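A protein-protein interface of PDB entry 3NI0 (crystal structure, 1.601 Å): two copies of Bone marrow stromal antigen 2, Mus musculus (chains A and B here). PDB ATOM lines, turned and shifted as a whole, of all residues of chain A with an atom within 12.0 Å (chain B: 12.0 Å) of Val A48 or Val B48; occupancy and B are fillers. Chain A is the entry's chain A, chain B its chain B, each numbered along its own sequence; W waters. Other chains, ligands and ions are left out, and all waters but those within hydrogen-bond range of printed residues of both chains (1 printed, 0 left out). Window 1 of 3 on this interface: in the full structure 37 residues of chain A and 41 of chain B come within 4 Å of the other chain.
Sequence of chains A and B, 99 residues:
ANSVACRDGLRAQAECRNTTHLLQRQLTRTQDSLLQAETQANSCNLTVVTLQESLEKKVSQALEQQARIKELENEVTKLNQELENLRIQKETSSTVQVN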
ATOM      1  N   THR A  39     -34.255 -19.186  -0.946  1.00  0.00           N
ATOM      2  CA  THR A  39     -33.100 -19.930  -0.448  1.00  0.00           C
ATOM      3  C   THR A  39     -31.830 -19.122  -0.694  1.00  0.00           C
ATOM      4  O   THR A  39     -30.959 -19.048   0.168  1.00  0.00           O
ATOM      5  CB  THR A  39     -32.975 -21.309  -1.127  1.00  0.00           C
ATOM      6  OG1 THR A  39     -34.081 -22.137  -0.746  1.00  0.00           O
ATOM      7  CG2 THR A  39     -31.686 -21.999  -0.717  1.00  0.00           C
ATOM      8  N   GLN A  40     -31.738 -18.515  -1.873  1.00  0.00           N
ATOM      9  CA  GLN A  40     -30.591 -17.683  -2.220  1.00  0.00           C
ATOM     10  C   GLN A  40     -30.512 -16.466  -1.305  1.00  0.00           C
ATOM     11  O   GLN A  40     -29.432 -16.101  -0.845  1.00  0.00           O
ATOM     12  CB  GLN A  40     -30.678 -17.237  -3.679  1.00  0.00           C
ATOM     13  CG  GLN A  40     -30.503 -18.372  -4.673  1.00  0.00           C
ATOM     14  CD  GLN A  40     -30.744 -17.939  -6.108  1.00  0.00           C
ATOM     15  OE1 GLN A  40     -30.901 -16.753  -6.393  1.00  0.00           O
ATOM     16  NE2 GLN A  40     -30.779 -18.906  -7.018  1.00  0.00           N
ATOM     17  N   ALA A  41     -31.657 -15.849  -1.035  1.00  0.00           N
ATOM     18  CA  ALA A  41     -31.706 -14.662  -0.190  1.00  0.00           C
ATOM     19  C   ALA A  41     -31.265 -15.003   1.227  1.00  0.00           C
ATOM     20  O   ALA A  41     -30.558 -14.227   1.868  1.00  0.00           O
ATOM     21  CB  ALA A  41     -33.106 -14.077  -0.182  1.00  0.00           C
ATOM     22  N   ASN A  42     -31.680 -16.171   1.708  1.00  0.00           N
ATOM     23  CA  ASN A  42     -31.332 -16.611   3.052  1.00  0.00           C
ATOM     24  C   ASN A  42     -29.831 -16.817   3.193  1.00  0.00           C
ATOM     25  O   ASN A  42     -29.232 -16.395   4.180  1.00  0.00           O
ATOM     26  CB  ASN A  42     -32.068 -17.909   3.394  1.00  0.00           C
ATOM     27  CG  ASN A  42     -31.805 -18.373   4.816  1.00  0.00           C
ATOM     28  OD1 ASN A  42     -31.922 -17.601   5.768  1.00  0.00           O
ATOM     29  ND2 ASN A  42     -31.438 -19.637   4.965  1.00  0.00           N
ATOM     30  N   SER A  43     -29.231 -17.467   2.201  1.00  0.00           N
ATOM     31  CA  SER A  43     -27.795 -17.723   2.214  1.00  0.00           C
ATOM     32  C   SER A  43     -27.023 -16.412   2.131  1.00  0.00           C
ATOM     33  O   SER A  43     -26.036 -16.213   2.839  1.00  0.00           O
ATOM     34  CB  SER A  43     -27.399 -18.631   1.048  1.00  0.00           C
ATOM     35  OG  SER A  43     -25.991 -18.800   0.997  1.00  0.00           O
ATOM     36  N   CYS A  44     -27.475 -15.522   1.254  1.00  0.00           N
ATOM     37  CA  CYS A  44     -26.845 -14.225   1.095  1.00  0.00           C
ATOM     38  C   CYS A  44     -26.868 -13.477   2.420  1.00  0.00           C
ATOM     39  O   CYS A  44     -25.898 -12.810   2.789  1.00  0.00           O
ATOM     40  CB  CYS A  44     -27.551 -13.406   0.013  1.00  0.00           C
ATOM     41  SG  CYS A  44     -26.770 -11.809  -0.270  1.00  0.00           S
ATOM     42  N   ASN A  45     -27.973 -13.589   3.147  1.00  0.00           N
ATOM     43  CA  ASN A  45     -28.100 -12.861   4.402  1.00  0.00           C
ATOM     44  C   ASN A  45     -27.080 -13.322   5.429  1.00  0.00           C
ATOM     45  O   ASN A  45     -26.581 -12.511   6.204  1.00  0.00           O
ATOM     46  CB  ASN A  45     -29.506 -12.984   4.987  1.00  0.00           C
ATOM     47  CG  ASN A  45     -29.651 -12.227   6.302  1.00  0.00           C
ATOM     48  OD1 ASN A  45     -29.731 -10.998   6.318  1.00  0.00           O
ATOM     49  ND2 ASN A  45     -29.661 -12.960   7.409  1.00  0.00           N
ATOM     50  N   LEU A  46     -26.766 -14.613   5.442  1.00  0.00           N
ATOM     51  CA  LEU A  46     -25.737 -15.110   6.350  1.00  0.00           C
ATOM     52  C   LEU A  46     -24.386 -14.530   5.951  1.00  0.00           C
ATOM     53  O   LEU A  46     -23.573 -14.197   6.807  1.00  0.00           O
ATOM     54  CB  LEU A  46     -25.675 -16.640   6.356  1.00  0.00           C
ATOM     55  CG  LEU A  46     -24.611 -17.217   7.298  1.00  0.00           C
ATOM     56  CD1 LEU A  46     -24.828 -16.751   8.726  1.00  0.00           C
ATOM     57  CD2 LEU A  46     -24.591 -18.739   7.226  1.00  0.00           C
ATOM     58  N   THR A  47     -24.154 -14.405   4.648  1.00  0.00           N
ATOM     59  CA  THR A  47     -22.901 -13.842   4.158  1.00  0.00           C
ATOM     60  C   THR A  47     -22.774 -12.394   4.609  1.00  0.00           C
ATOM     61  O   THR A  47     -21.694 -11.943   4.984  1.00  0.00           O
ATOM     62  CB  THR A  47     -22.801 -13.914   2.626  1.00  0.00           C
ATOM     63  OG1 THR A  47     -22.905 -15.277   2.202  1.00  0.00           O
ATOM     64  CG2 THR A  47     -21.475 -13.337   2.150  1.00  0.00           C
ATOM     65  N   VAL A  48     -23.890 -11.673   4.580  1.00  0.00           N
ATOM     66  CA  VAL A  48     -23.915 -10.288   5.029  1.00  0.00           C
ATOM     67  C   VAL A  48     -23.567 -10.196   6.510  1.00  0.00           C
ATOM     68  O   VAL A  48     -22.759  -9.363   6.911  1.00  0.00           O
ATOM     69  CB  VAL A  48     -25.292  -9.643   4.784  1.00  0.00           C
ATOM     70  CG1 VAL A  48     -25.432  -8.347   5.575  1.00  0.00           C
ATOM     71  CG2 VAL A  48     -25.503  -9.393   3.300  1.00  0.00           C
ATOM     72  N   VAL A  49     -24.182 -11.054   7.318  1.00  0.00           N
ATOM     73  CA  VAL A  49     -23.926 -11.069   8.756  1.00  0.00           C
ATOM     74  C   VAL A  49     -22.472 -11.413   9.064  1.00  0.00           C
ATOM     75  O   VAL A  49     -21.878 -10.853   9.983  1.00  0.00           O
ATOM     76  CB  VAL A  49     -24.840 -12.075   9.482  1.00  0.00           C
ATOM     77  CG1 VAL A  49     -24.315 -12.356  10.887  1.00  0.00           C
ATOM     78  CG2 VAL A  49     -26.267 -11.558   9.530  1.00  0.00           C
ATOM     79  N   THR A  50     -21.903 -12.335   8.295  1.00  0.00           N
ATOM     80  CA  THR A  50     -20.530 -12.768   8.510  1.00  0.00           C
ATOM     81  C   THR A  50     -19.564 -11.633   8.173  1.00  0.00           C
ATOM     82  O   THR A  50     -18.566 -11.427   8.865  1.00  0.00           O
ATOM     83  CB  THR A  50     -20.183 -14.011   7.662  1.00  0.00           C
ATOM     84  OG1 THR A  50     -21.066 -15.091   7.999  1.00  0.00           O
ATOM     85  CG2 THR A  50     -18.747 -14.447   7.911  1.00  0.00           C
ATOM     86  N   LEU A  51     -19.868 -10.893   7.110  1.00  0.00           N
ATOM     87  CA  LEU A  51     -19.048  -9.753   6.711  1.00  0.00           C
ATOM     88  C   LEU A  51     -19.164  -8.619   7.722  1.00  0.00           C
ATOM     89  O   LEU A  51     -18.180  -7.948   8.023  1.00  0.00           O
ATOM     90  CB  LEU A  51     -19.454  -9.258   5.323  1.00  0.00           C
ATOM     91  CG  LEU A  51     -18.978 -10.128   4.161  1.00  0.00           C
ATOM     92  CD1 LEU A  51     -19.793  -9.841   2.902  1.00  0.00           C
ATOM     93  CD2 LEU A  51     -17.495  -9.919   3.908  1.00  0.00           C
ATOM     94  N   GLN A  52     -20.369  -8.407   8.240  1.00  0.00           N
ATOM     95  CA  GLN A  52     -20.597  -7.382   9.252  1.00  0.00           C
ATOM     96  C   GLN A  52     -19.837  -7.717  10.531  1.00  0.00           C
ATOM     97  O   GLN A  52     -19.300  -6.831  11.190  1.00  0.00           O
ATOM     98  CB  GLN A  52     -22.093  -7.236   9.537  1.00  0.00           C
ATOM     99  CG  GLN A  52     -22.841  -6.449   8.473  1.00  0.00           C
ATOM    100  CD  GLN A  52     -24.348  -6.507   8.641  1.00  0.00           C
ATOM    101  OE1 GLN A  52     -24.892  -7.496   9.127  1.00  0.00           O
ATOM    102  NE2 GLN A  52     -25.030  -5.442   8.233  1.00  0.00           N
ATOM    103  N   GLU A  53     -19.788  -8.999  10.876  1.00  0.00           N
ATOM    104  CA  GLU A  53     -19.037  -9.448  12.048  1.00  0.00           C
ATOM    105  C   GLU A  53     -17.552  -9.159  11.883  1.00  0.00           C
ATOM    106  O   GLU A  53     -16.885  -8.709  12.816  1.00  0.00           O
ATOM    107  CB  GLU A  53     -19.239 -10.945  12.270  1.00  0.00           C
ATOM    108  CG  GLU A  53     -20.599 -11.311  12.825  1.00  0.00           C
ATOM    109  CD  GLU A  53     -20.883 -12.793  12.737  1.00  0.00           C
ATOM    110  OE1 GLU A  53     -20.094 -13.523  12.098  1.00  0.00           O
ATOM    111  OE2 GLU A  53     -21.900 -13.227  13.310  1.00  0.00           O
ATOM    112  N   SER A  54     -17.037  -9.419  10.688  1.00  0.00           N
ATOM    113  CA  SER A  54     -15.617  -9.237  10.411  1.00  0.00           C
ATOM    114  C   SER A  54     -15.255  -7.760  10.351  1.00  0.00           C
ATOM    115  O   SER A  54     -14.175  -7.361  10.783  1.00  0.00           O
ATOM    116  CB  SER A  54     -15.244  -9.912   9.094  1.00  0.00           C
ATOM    117  OG  SER A  54     -13.875  -9.710   8.785  1.00  0.00           O
ATOM    118  N   LEU A  55     -16.169  -6.955   9.820  1.00  0.00           N
ATOM    119  CA  LEU A  55     -15.936  -5.528   9.663  1.00  0.00           C
ATOM    120  C   LEU A  55     -15.899  -4.850  11.027  1.00  0.00           C
ATOM    121  O   LEU A  55     -15.085  -3.961  11.262  1.00  0.00           O
ATOM    122  CB  LEU A  55     -17.023  -4.896   8.795  1.00  0.00           C
ATOM    123  CG  LEU A  55     -16.829  -3.414   8.473  1.00  0.00           C
ATOM    124  CD1 LEU A  55     -15.528  -3.200   7.707  1.00  0.00           C
ATOM    125  CD2 LEU A  55     -18.007  -2.869   7.686  1.00  0.00           C
ATOM    126  N   GLU A  56     -16.788  -5.269  11.921  1.00  0.00           N
ATOM    127  CA  GLU A  56     -16.823  -4.731  13.276  1.00  0.00           C
ATOM    128  C   GLU A  56     -15.484  -4.959  13.965  1.00  0.00           C
ATOM    129  O   GLU A  56     -14.946  -4.061  14.613  1.00  0.00           O
ATOM    130  CB  GLU A  56     -17.945  -5.394  14.076  1.00  0.00           C
ATOM    131  CG  GLU A  56     -18.079  -4.886  15.503  1.00  0.00           C
ATOM    132  CD  GLU A  56     -19.338  -5.387  16.186  1.00  0.00           C
ATOM    133  OE1 GLU A  56     -19.357  -6.555  16.625  1.00  0.00           O
ATOM    134  OE2 GLU A  56     -20.313  -4.612  16.280  1.00  0.00           O
ATOM    135  N   LYS A  57     -14.948  -6.166  13.820  1.00  0.00           N
ATOM    136  CA  LYS A  57     -13.670  -6.518  14.426  1.00  0.00           C
ATOM    137  C   LYS A  57     -12.550  -5.634  13.882  1.00  0.00           C
ATOM    138  O   LYS A  57     -11.709  -5.151  14.637  1.00  0.00           O
ATOM    139  CB  LYS A  57     -13.347  -7.989  14.161  1.00  0.00           C
ATOM    140  CG  LYS A  57     -12.233  -8.553  15.028  1.00  0.00           C
ATOM    141  CD  LYS A  57     -12.131 -10.064  14.869  1.00  0.00           C
ATOM    142  CE  LYS A  57     -11.428 -10.714  16.054  1.00  0.00           C
ATOM    143  NZ  LYS A  57     -10.030 -10.234  16.231  1.00  0.00           N
ATOM    144  N   GLU B  38     -36.563 -12.106  -5.663  1.00  0.00           N
ATOM    145  CA  GLU B  38     -35.400 -11.857  -6.501  1.00  0.00           C
ATOM    146  C   GLU B  38     -34.794 -10.502  -6.157  1.00  0.00           C
ATOM    147  O   GLU B  38     -33.573 -10.351  -6.117  1.00  0.00           O
ATOM    148  CB  GLU B  38     -35.784 -11.940  -7.978  1.00  0.00           C
ATOM    149  CG  GLU B  38     -35.918 -13.373  -8.475  1.00  0.00           C
ATOM    150  CD  GLU B  38     -36.588 -13.479  -9.840  1.00  0.00           C
ATOM    151  OE1 GLU B  38     -37.366 -12.571 -10.211  1.00  0.00           O
ATOM    152  OE2 GLU B  38     -36.354 -14.492 -10.534  1.00  0.00           O
ATOM    153  N   THR B  39     -35.651  -9.526  -5.886  1.00  0.00           N
ATOM    154  CA  THR B  39     -35.188  -8.202  -5.489  1.00  0.00           C
ATOM    155  C   THR B  39     -34.520  -8.238  -4.118  1.00  0.00           C
ATOM    156  O   THR B  39     -33.535  -7.544  -3.892  1.00  0.00           O
ATOM    157  CB  THR B  39     -36.333  -7.176  -5.476  1.00  0.00           C
ATOM    158  OG1 THR B  39     -36.796  -6.968  -6.813  1.00  0.00           O
ATOM    159  CG2 THR B  39     -35.866  -5.846  -4.897  1.00  0.00           C
ATOM    160  N   GLN B  40     -35.044  -9.046  -3.200  1.00  0.00           N
ATOM    161  CA  GLN B  40     -34.392  -9.187  -1.905  1.00  0.00           C
ATOM    162  C   GLN B  40     -32.989  -9.749  -2.107  1.00  0.00           C
ATOM    163  O   GLN B  40     -32.039  -9.310  -1.466  1.00  0.00           O
ATOM    164  CB  GLN B  40     -35.182 -10.090  -0.955  1.00  0.00           C
ATOM    165  CG  GLN B  40     -34.510 -10.213   0.411  1.00  0.00           C
ATOM    166  CD  GLN B  40     -35.223 -11.157   1.356  1.00  0.00           C
ATOM    167  OE1 GLN B  40     -36.388 -11.502   1.151  1.00  0.00           O
ATOM    168  NE2 GLN B  40     -34.523 -11.583   2.403  1.00  0.00           N
ATOM    169  N   ALA B  41     -32.867 -10.718  -3.007  1.00  0.00           N
ATOM    170  CA  ALA B  41     -31.577 -11.342  -3.284  1.00  0.00           C
ATOM    171  C   ALA B  41     -30.625 -10.356  -3.958  1.00  0.00           C
ATOM    172  O   ALA B  41     -29.431 -10.351  -3.670  1.00  0.00           O
ATOM    173  CB  ALA B  41     -31.760 -12.575  -4.146  1.00  0.00           C
ATOM    174  N   ASN B  42     -31.155  -9.516  -4.844  1.00  0.00           N
ATOM    175  CA  ASN B  42     -30.328  -8.539  -5.549  1.00  0.00           C
ATOM    176  C   ASN B  42     -29.839  -7.444  -4.617  1.00  0.00           C
ATOM    177  O   ASN B  42     -28.700  -6.996  -4.717  1.00  0.00           O
ATOM    178  CB  ASN B  42     -31.095  -7.910  -6.710  1.00  0.00           C
ATOM    179  CG  ASN B  42     -31.342  -8.886  -7.842  1.00  0.00           C
ATOM    180  OD1 ASN B  42     -30.606  -9.859  -8.008  1.00  0.00           O
ATOM    181  ND2 ASN B  42     -32.379  -8.629  -8.630  1.00  0.00           N
ATOM    182  N   SER B  43     -30.715  -7.001  -3.723  1.00  0.00           N
ATOM    183  CA  SER B  43     -30.351  -5.999  -2.729  1.00  0.00           C
ATOM    184  C   SER B  43     -29.294  -6.572  -1.802  1.00  0.00           C
ATOM    185  O   SER B  43     -28.325  -5.896  -1.460  1.00  0.00           O
ATOM    186  CB  SER B  43     -31.575  -5.562  -1.923  1.00  0.00           C
ATOM    187  OG  SER B  43     -31.213  -4.666  -0.885  1.00  0.00           O
ATOM    188  N   CYS B  44     -29.482  -7.824  -1.401  1.00  0.00           N
ATOM    189  CA  CYS B  44     -28.525  -8.490  -0.529  1.00  0.00           C
ATOM    190  C   CYS B  44     -27.178  -8.615  -1.228  1.00  0.00           C
ATOM    191  O   CYS B  44     -26.136  -8.483  -0.597  1.00  0.00           O
ATOM    192  CB  CYS B  44     -29.025  -9.874  -0.114  1.00  0.00           C
ATOM    193  SG  CYS B  44     -27.905 -10.727   1.022  1.00  0.00           S
ATOM    194  N   ASN B  45     -27.199  -8.862  -2.534  1.00  0.00           N
ATOM    195  CA  ASN B  45     -25.958  -8.960  -3.293  1.00  0.00           C
ATOM    196  C   ASN B  45     -25.194  -7.640  -3.272  1.00  0.00           C
ATOM    197  O   ASN B  45     -23.968  -7.628  -3.168  1.00  0.00           O
ATOM    198  CB  ASN B  45     -26.229  -9.403  -4.734  1.00  0.00           C
ATOM    199  CG  ASN B  45     -26.574 -10.880  -4.835  1.00  0.00           C
ATOM    200  OD1 ASN B  45     -26.198 -11.678  -3.977  1.00  0.00           O
ATOM    201  ND2 ASN B  45     -27.287 -11.253  -5.893  1.00  0.00           N
ATOM    202  N   LEU B  46     -25.922  -6.532  -3.360  1.00  0.00           N
ATOM    203  CA  LEU B  46     -25.307  -5.211  -3.292  1.00  0.00           C
ATOM    204  C   LEU B  46     -24.699  -4.954  -1.923  1.00  0.00           C
ATOM    205  O   LEU B  46     -23.618  -4.382  -1.820  1.00  0.00           O
ATOM    206  CB  LEU B  46     -26.331  -4.119  -3.595  1.00  0.00           C
ATOM    207  CG  LEU B  46     -26.761  -4.001  -5.054  1.00  0.00           C
ATOM    208  CD1 LEU B  46     -27.671  -2.794  -5.240  1.00  0.00           C
ATOM    209  CD2 LEU B  46     -25.542  -3.897  -5.958  1.00  0.00           C
ATOM    210  N   THR B  47     -25.403  -5.368  -0.876  1.00  0.00           N
ATOM    211  CA  THR B  47     -24.924  -5.193   0.487  1.00  0.00           C
ATOM    212  C   THR B  47     -23.637  -5.980   0.690  1.00  0.00           C
ATOM    213  O   THR B  47     -22.721  -5.520   1.370  1.00  0.00           O
ATOM    214  CB  THR B  47     -25.977  -5.648   1.514  1.00  0.00           C
ATOM    215  OG1 THR B  47     -27.179  -4.884   1.337  1.00  0.00           O
ATOM    216  CG2 THR B  47     -25.460  -5.458   2.931  1.00  0.00           C
ATOM    217  N   VAL B  48     -23.570  -7.166   0.095  1.00  0.00           N
ATOM    218  CA  VAL B  48     -22.370  -7.989   0.176  1.00  0.00           C
ATOM    219  C   VAL B  48     -21.191  -7.274  -0.473  1.00  0.00           C
ATOM    220  O   VAL B  48     -20.109  -7.212   0.100  1.00  0.00           O
ATOM    221  CB  VAL B  48     -22.563  -9.364  -0.492  1.00  0.00           C
ATOM    222  CG1 VAL B  48     -21.222 -10.054  -0.691  1.00  0.00           C
ATOM    223  CG2 VAL B  48     -23.495 -10.232   0.339  1.00  0.00           C
ATOM    224  N   VAL B  49     -21.399  -6.732  -1.670  1.00  0.00           N
ATOM    225  CA  VAL B  49     -20.334  -6.017  -2.368  1.00  0.00           C
ATOM    226  C   VAL B  49     -19.885  -4.798  -1.564  1.00  0.00           C
ATOM    227  O   VAL B  49     -18.689  -4.543  -1.427  1.00  0.00           O
ATOM    228  CB  VAL B  49     -20.771  -5.560  -3.771  1.00  0.00           C
ATOM    229  CG1 VAL B  49     -19.683  -4.706  -4.414  1.00  0.00           C
ATOM    230  CG2 VAL B  49     -21.093  -6.761  -4.650  1.00  0.00           C
ATOM    231  N   THR B  50     -20.848  -4.047  -1.040  1.00  0.00           N
ATOM    232  CA  THR B  50     -20.549  -2.881  -0.214  1.00  0.00           C
ATOM    233  C   THR B  50     -19.650  -3.262   0.953  1.00  0.00           C
ATOM    234  O   THR B  50     -18.631  -2.619   1.198  1.00  0.00           O
ATOM    235  CB  THR B  50     -21.836  -2.246   0.349  1.00  0.00           C
ATOM    236  OG1 THR B  50     -22.655  -1.774  -0.728  1.00  0.00           O
ATOM    237  CG2 THR B  50     -21.503  -1.084   1.274  1.00  0.00           C
ATOM    238  N   LEU B  51     -20.035  -4.315   1.664  1.00  0.00           N
ATOM    239  CA  LEU B  51     -19.314  -4.754   2.853  1.00  0.00           C
ATOM    240  C   LEU B  51     -17.950  -5.340   2.510  1.00  0.00           C
ATOM    241  O   LEU B  51     -16.994  -5.164   3.256  1.00  0.00           O
ATOM    242  CB  LEU B  51     -20.137  -5.789   3.619  1.00  0.00           C
ATOM    243  CG  LEU B  51     -21.334  -5.225   4.380  1.00  0.00           C
ATOM    244  CD1 LEU B  51     -22.261  -6.349   4.830  1.00  0.00           C
ATOM    245  CD2 LEU B  51     -20.865  -4.399   5.566  1.00  0.00           C
ATOM    246  N   GLN B  52     -17.865  -6.039   1.383  1.00  0.00           N
ATOM    247  CA  GLN B  52     -16.596  -6.600   0.937  1.00  0.00           C
ATOM    248  C   GLN B  52     -15.592  -5.488   0.682  1.00  0.00           C
ATOM    249  O   GLN B  52     -14.423  -5.603   1.043  1.00  0.00           O
ATOM    250  CB  GLN B  52     -16.777  -7.425  -0.336  1.00  0.00           C
ATOM    251  CG  GLN B  52     -17.307  -8.829  -0.104  1.00  0.00           C
ATOM    252  CD  GLN B  52     -17.430  -9.617  -1.395  1.00  0.00           C
ATOM    253  OE1 GLN B  52     -18.189  -9.245  -2.290  1.00  0.00           O
ATOM    254  NE2 GLN B  52     -16.674 -10.705  -1.501  1.00  0.00           N
ATOM    255  N   GLU B  53     -16.056  -4.407   0.067  1.00  0.00           N
ATOM    256  CA  GLU B  53     -15.168  -3.304  -0.285  1.00  0.00           C
ATOM    257  C   GLU B  53     -14.768  -2.495   0.943  1.00  0.00           C
ATOM    258  O   GLU B  53     -13.628  -2.049   1.046  1.00  0.00           O
ATOM    259  CB  GLU B  53     -15.804  -2.419  -1.358  1.00  0.00           C
ATOM    260  CG  GLU B  53     -15.879  -3.115  -2.718  1.00  0.00           C
ATOM    261  CD  GLU B  53     -16.330  -2.201  -3.844  1.00  0.00           C
ATOM    262  OE1 GLU B  53     -16.178  -0.968  -3.716  1.00  0.00           O
ATOM    263  OE2 GLU B  53     -16.831  -2.721  -4.865  1.00  0.00           O
ATOM    264  N   SER B  54     -15.695  -2.315   1.879  1.00  0.00           N
ATOM    265  CA  SER B  54     -15.372  -1.661   3.148  1.00  0.00           C
ATOM    266  C   SER B  54     -14.369  -2.490   3.943  1.00  0.00           C
ATOM    267  O   SER B  54     -13.441  -1.949   4.542  1.00  0.00           O
ATOM    268  CB  SER B  54     -16.635  -1.445   3.986  1.00  0.00           C
ATOM    269  OG  SER B  54     -17.469  -0.456   3.413  1.00  0.00           O
ATOM    270  N   LEU B  55     -14.561  -3.805   3.937  1.00  0.00           N
ATOM    271  CA  LEU B  55     -13.700  -4.717   4.676  1.00  0.00           C
ATOM    272  C   LEU B  55     -12.303  -4.742   4.071  1.00  0.00           C
ATOM    273  O   LEU B  55     -11.313  -4.824   4.794  1.00  0.00           O
ATOM    274  CB  LEU B  55     -14.292  -6.129   4.691  1.00  0.00           C
ATOM    275  CG  LEU B  55     -13.514  -7.167   5.509  1.00  0.00           C
ATOM    276  CD1 LEU B  55     -13.322  -6.704   6.946  1.00  0.00           C
ATOM    277  CD2 LEU B  55     -14.217  -8.518   5.474  1.00  0.00           C
ATOM    278  N   GLU B  56     -12.222  -4.667   2.746  1.00  0.00           N
ATOM    279  CA  GLU B  56     -10.931  -4.637   2.068  1.00  0.00           C
ATOM    280  C   GLU B  56     -10.158  -3.382   2.457  1.00  0.00           C
ATOM    281  O   GLU B  56      -8.953  -3.439   2.691  1.00  0.00           O
ATOM    282  CB  GLU B  56     -11.108  -4.697   0.551  1.00  0.00           C
ATOM    283  CG  GLU B  56     -11.545  -6.065   0.038  1.00  0.00           C
ATOM    284  CD  GLU B  56     -11.940  -6.042  -1.423  1.00  0.00           C
ATOM    285  OE1 GLU B  56     -11.447  -5.161  -2.159  1.00  0.00           O
ATOM    286  OE2 GLU B  56     -12.748  -6.901  -1.835  1.00  0.00           O
ATOM    287  N   LYS B  57     -10.853  -2.251   2.529  1.00  0.00           N
ATOM    288  CA  LYS B  57     -10.206  -0.994   2.901  1.00  0.00           C
ATOM    289  C   LYS B  57      -9.751  -1.010   4.355  1.00  0.00           C
ATOM    290  O   LYS B  57      -8.695  -0.473   4.680  1.00  0.00           O
ATOM    291  CB  LYS B  57     -11.135   0.201   2.674  1.00  0.00           C
ATOM    292  CG  LYS B  57     -11.515   0.440   1.221  1.00  0.00           C
ATOM    293  CD  LYS B  57     -10.305   0.529   0.309  1.00  0.00           C
ATOM    294  CE  LYS B  57      -9.546   1.832   0.481  1.00  0.00           C
ATOM    295  NZ  LYS B  57      -8.779   2.150  -0.762  1.00  0.00           N
HETATM  296  O   HOH W   1     -31.558 -11.473   2.136  1.00  0.00           O
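The side-chain sulfur (SG) of Cys B44 sits at hydrogen-bond distance from the backbone NH (N) of Asn A45, 3.6 Å away.
The side-chain sulfur (SG) of Cys A44 forms a disulfide with the side-chain sulfur (SG) of Cys B44 (2.0 Å).
SG of Cys A44 sits at hydrogen-bond distance from N of Asn B45 (3.7 Å).
The side-chain amide nitrogen (ND2) of Asn B45 sits close to the backbone carbonyl oxygen (O) of Ala B41, at 3.2 Å.
OG of Ser B54 is in hydrogen-bond range of O of Thr B50 (3.3 Å).
The backbone carbonyl oxygen (O) of Ser B43 is in hydrogen-bond range of the side-chain hydroxyl (OG1) of Thr B47, 3.2 Å away.
Among the printed residues, merely in contact across the chains: Ser A54 with Leu B55, Val A48 with Cys B44, Val A48 with Val B48, Cys A44 with Val B48, Gln A52 with Leu B51, Val A48 with Leu B51, Leu A55 with Leu B55, Leu A51 with Val B48, Ala A41 with Gln B40, Leu A55 with Leu B51, Leu A51 with Leu B55, Val A48 with Thr B47, Leu A51 with Leu B51 and Leu A55 with Ser B54.
Of chain B, only Cys B44 comes within 4 Å of Asn A45.
No residue of chain B comes within 4 Å of Leu A46.
No residue of chain B comes within 4 Å of Thr A47.
No residue of chain B comes within 4 Å of Thr A50.
Gln A52 touches one residue of chain B.
Printed residues of chain A within 4 Å of Gln B40: Ala A41.
Ser B43 touches none of the printed residues of chain A.
Cys B44 touches three residues of chain A.
Of chain A, only Cys A44 (3.7 Å) comes within 4 Å of Asn B45.
Thr B47 touches just one residue of chain A: Val A48.
Of chain A, only Cys A44 (3.7 Å), Val A48 (3.7 Å) and Leu A51 (3.9 Å) come within 4 Å of Val B48.
No residue of chain A comes within 4 Å of Val B49.
No residue of chain A comes within 4 Å of Thr B50.
Of the printed residues of chain A, Ser B54 touches Leu A55.
Printed residues of chain A that touch a printed residue of chain B: Ala A41, Cys A44, Asn A45, Val A48, Leu A51, Gln A52, Ser A54 and Leu A55.
Of the 20 printed residues of chain B, 8 touch a printed residue of chain A.
Cys B44 touches its own counterpart, Cys A44.
Val A48 touches its own counterpart, Val B48.
Val A48 touches Leu B51, and with the chains exchanged Leu A51 touches Val B48.
Leu A55 touches its own counterpart, Leu B55.
Positions printed for both chains: 39, 40, 41, 42, 43, 44, 45, 46, 47, 48, 49, 50, 51, 52, 53, 54, 55, 56 and 57.
Of the 17 pairs that touch across the chains among the printed residues, 14 have their exchanged pair printed and touching as well.
Water W1 bridges the backbone carbonyl oxygen of Ala A41 and the side-chain amide nitrogen of Gln B40.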
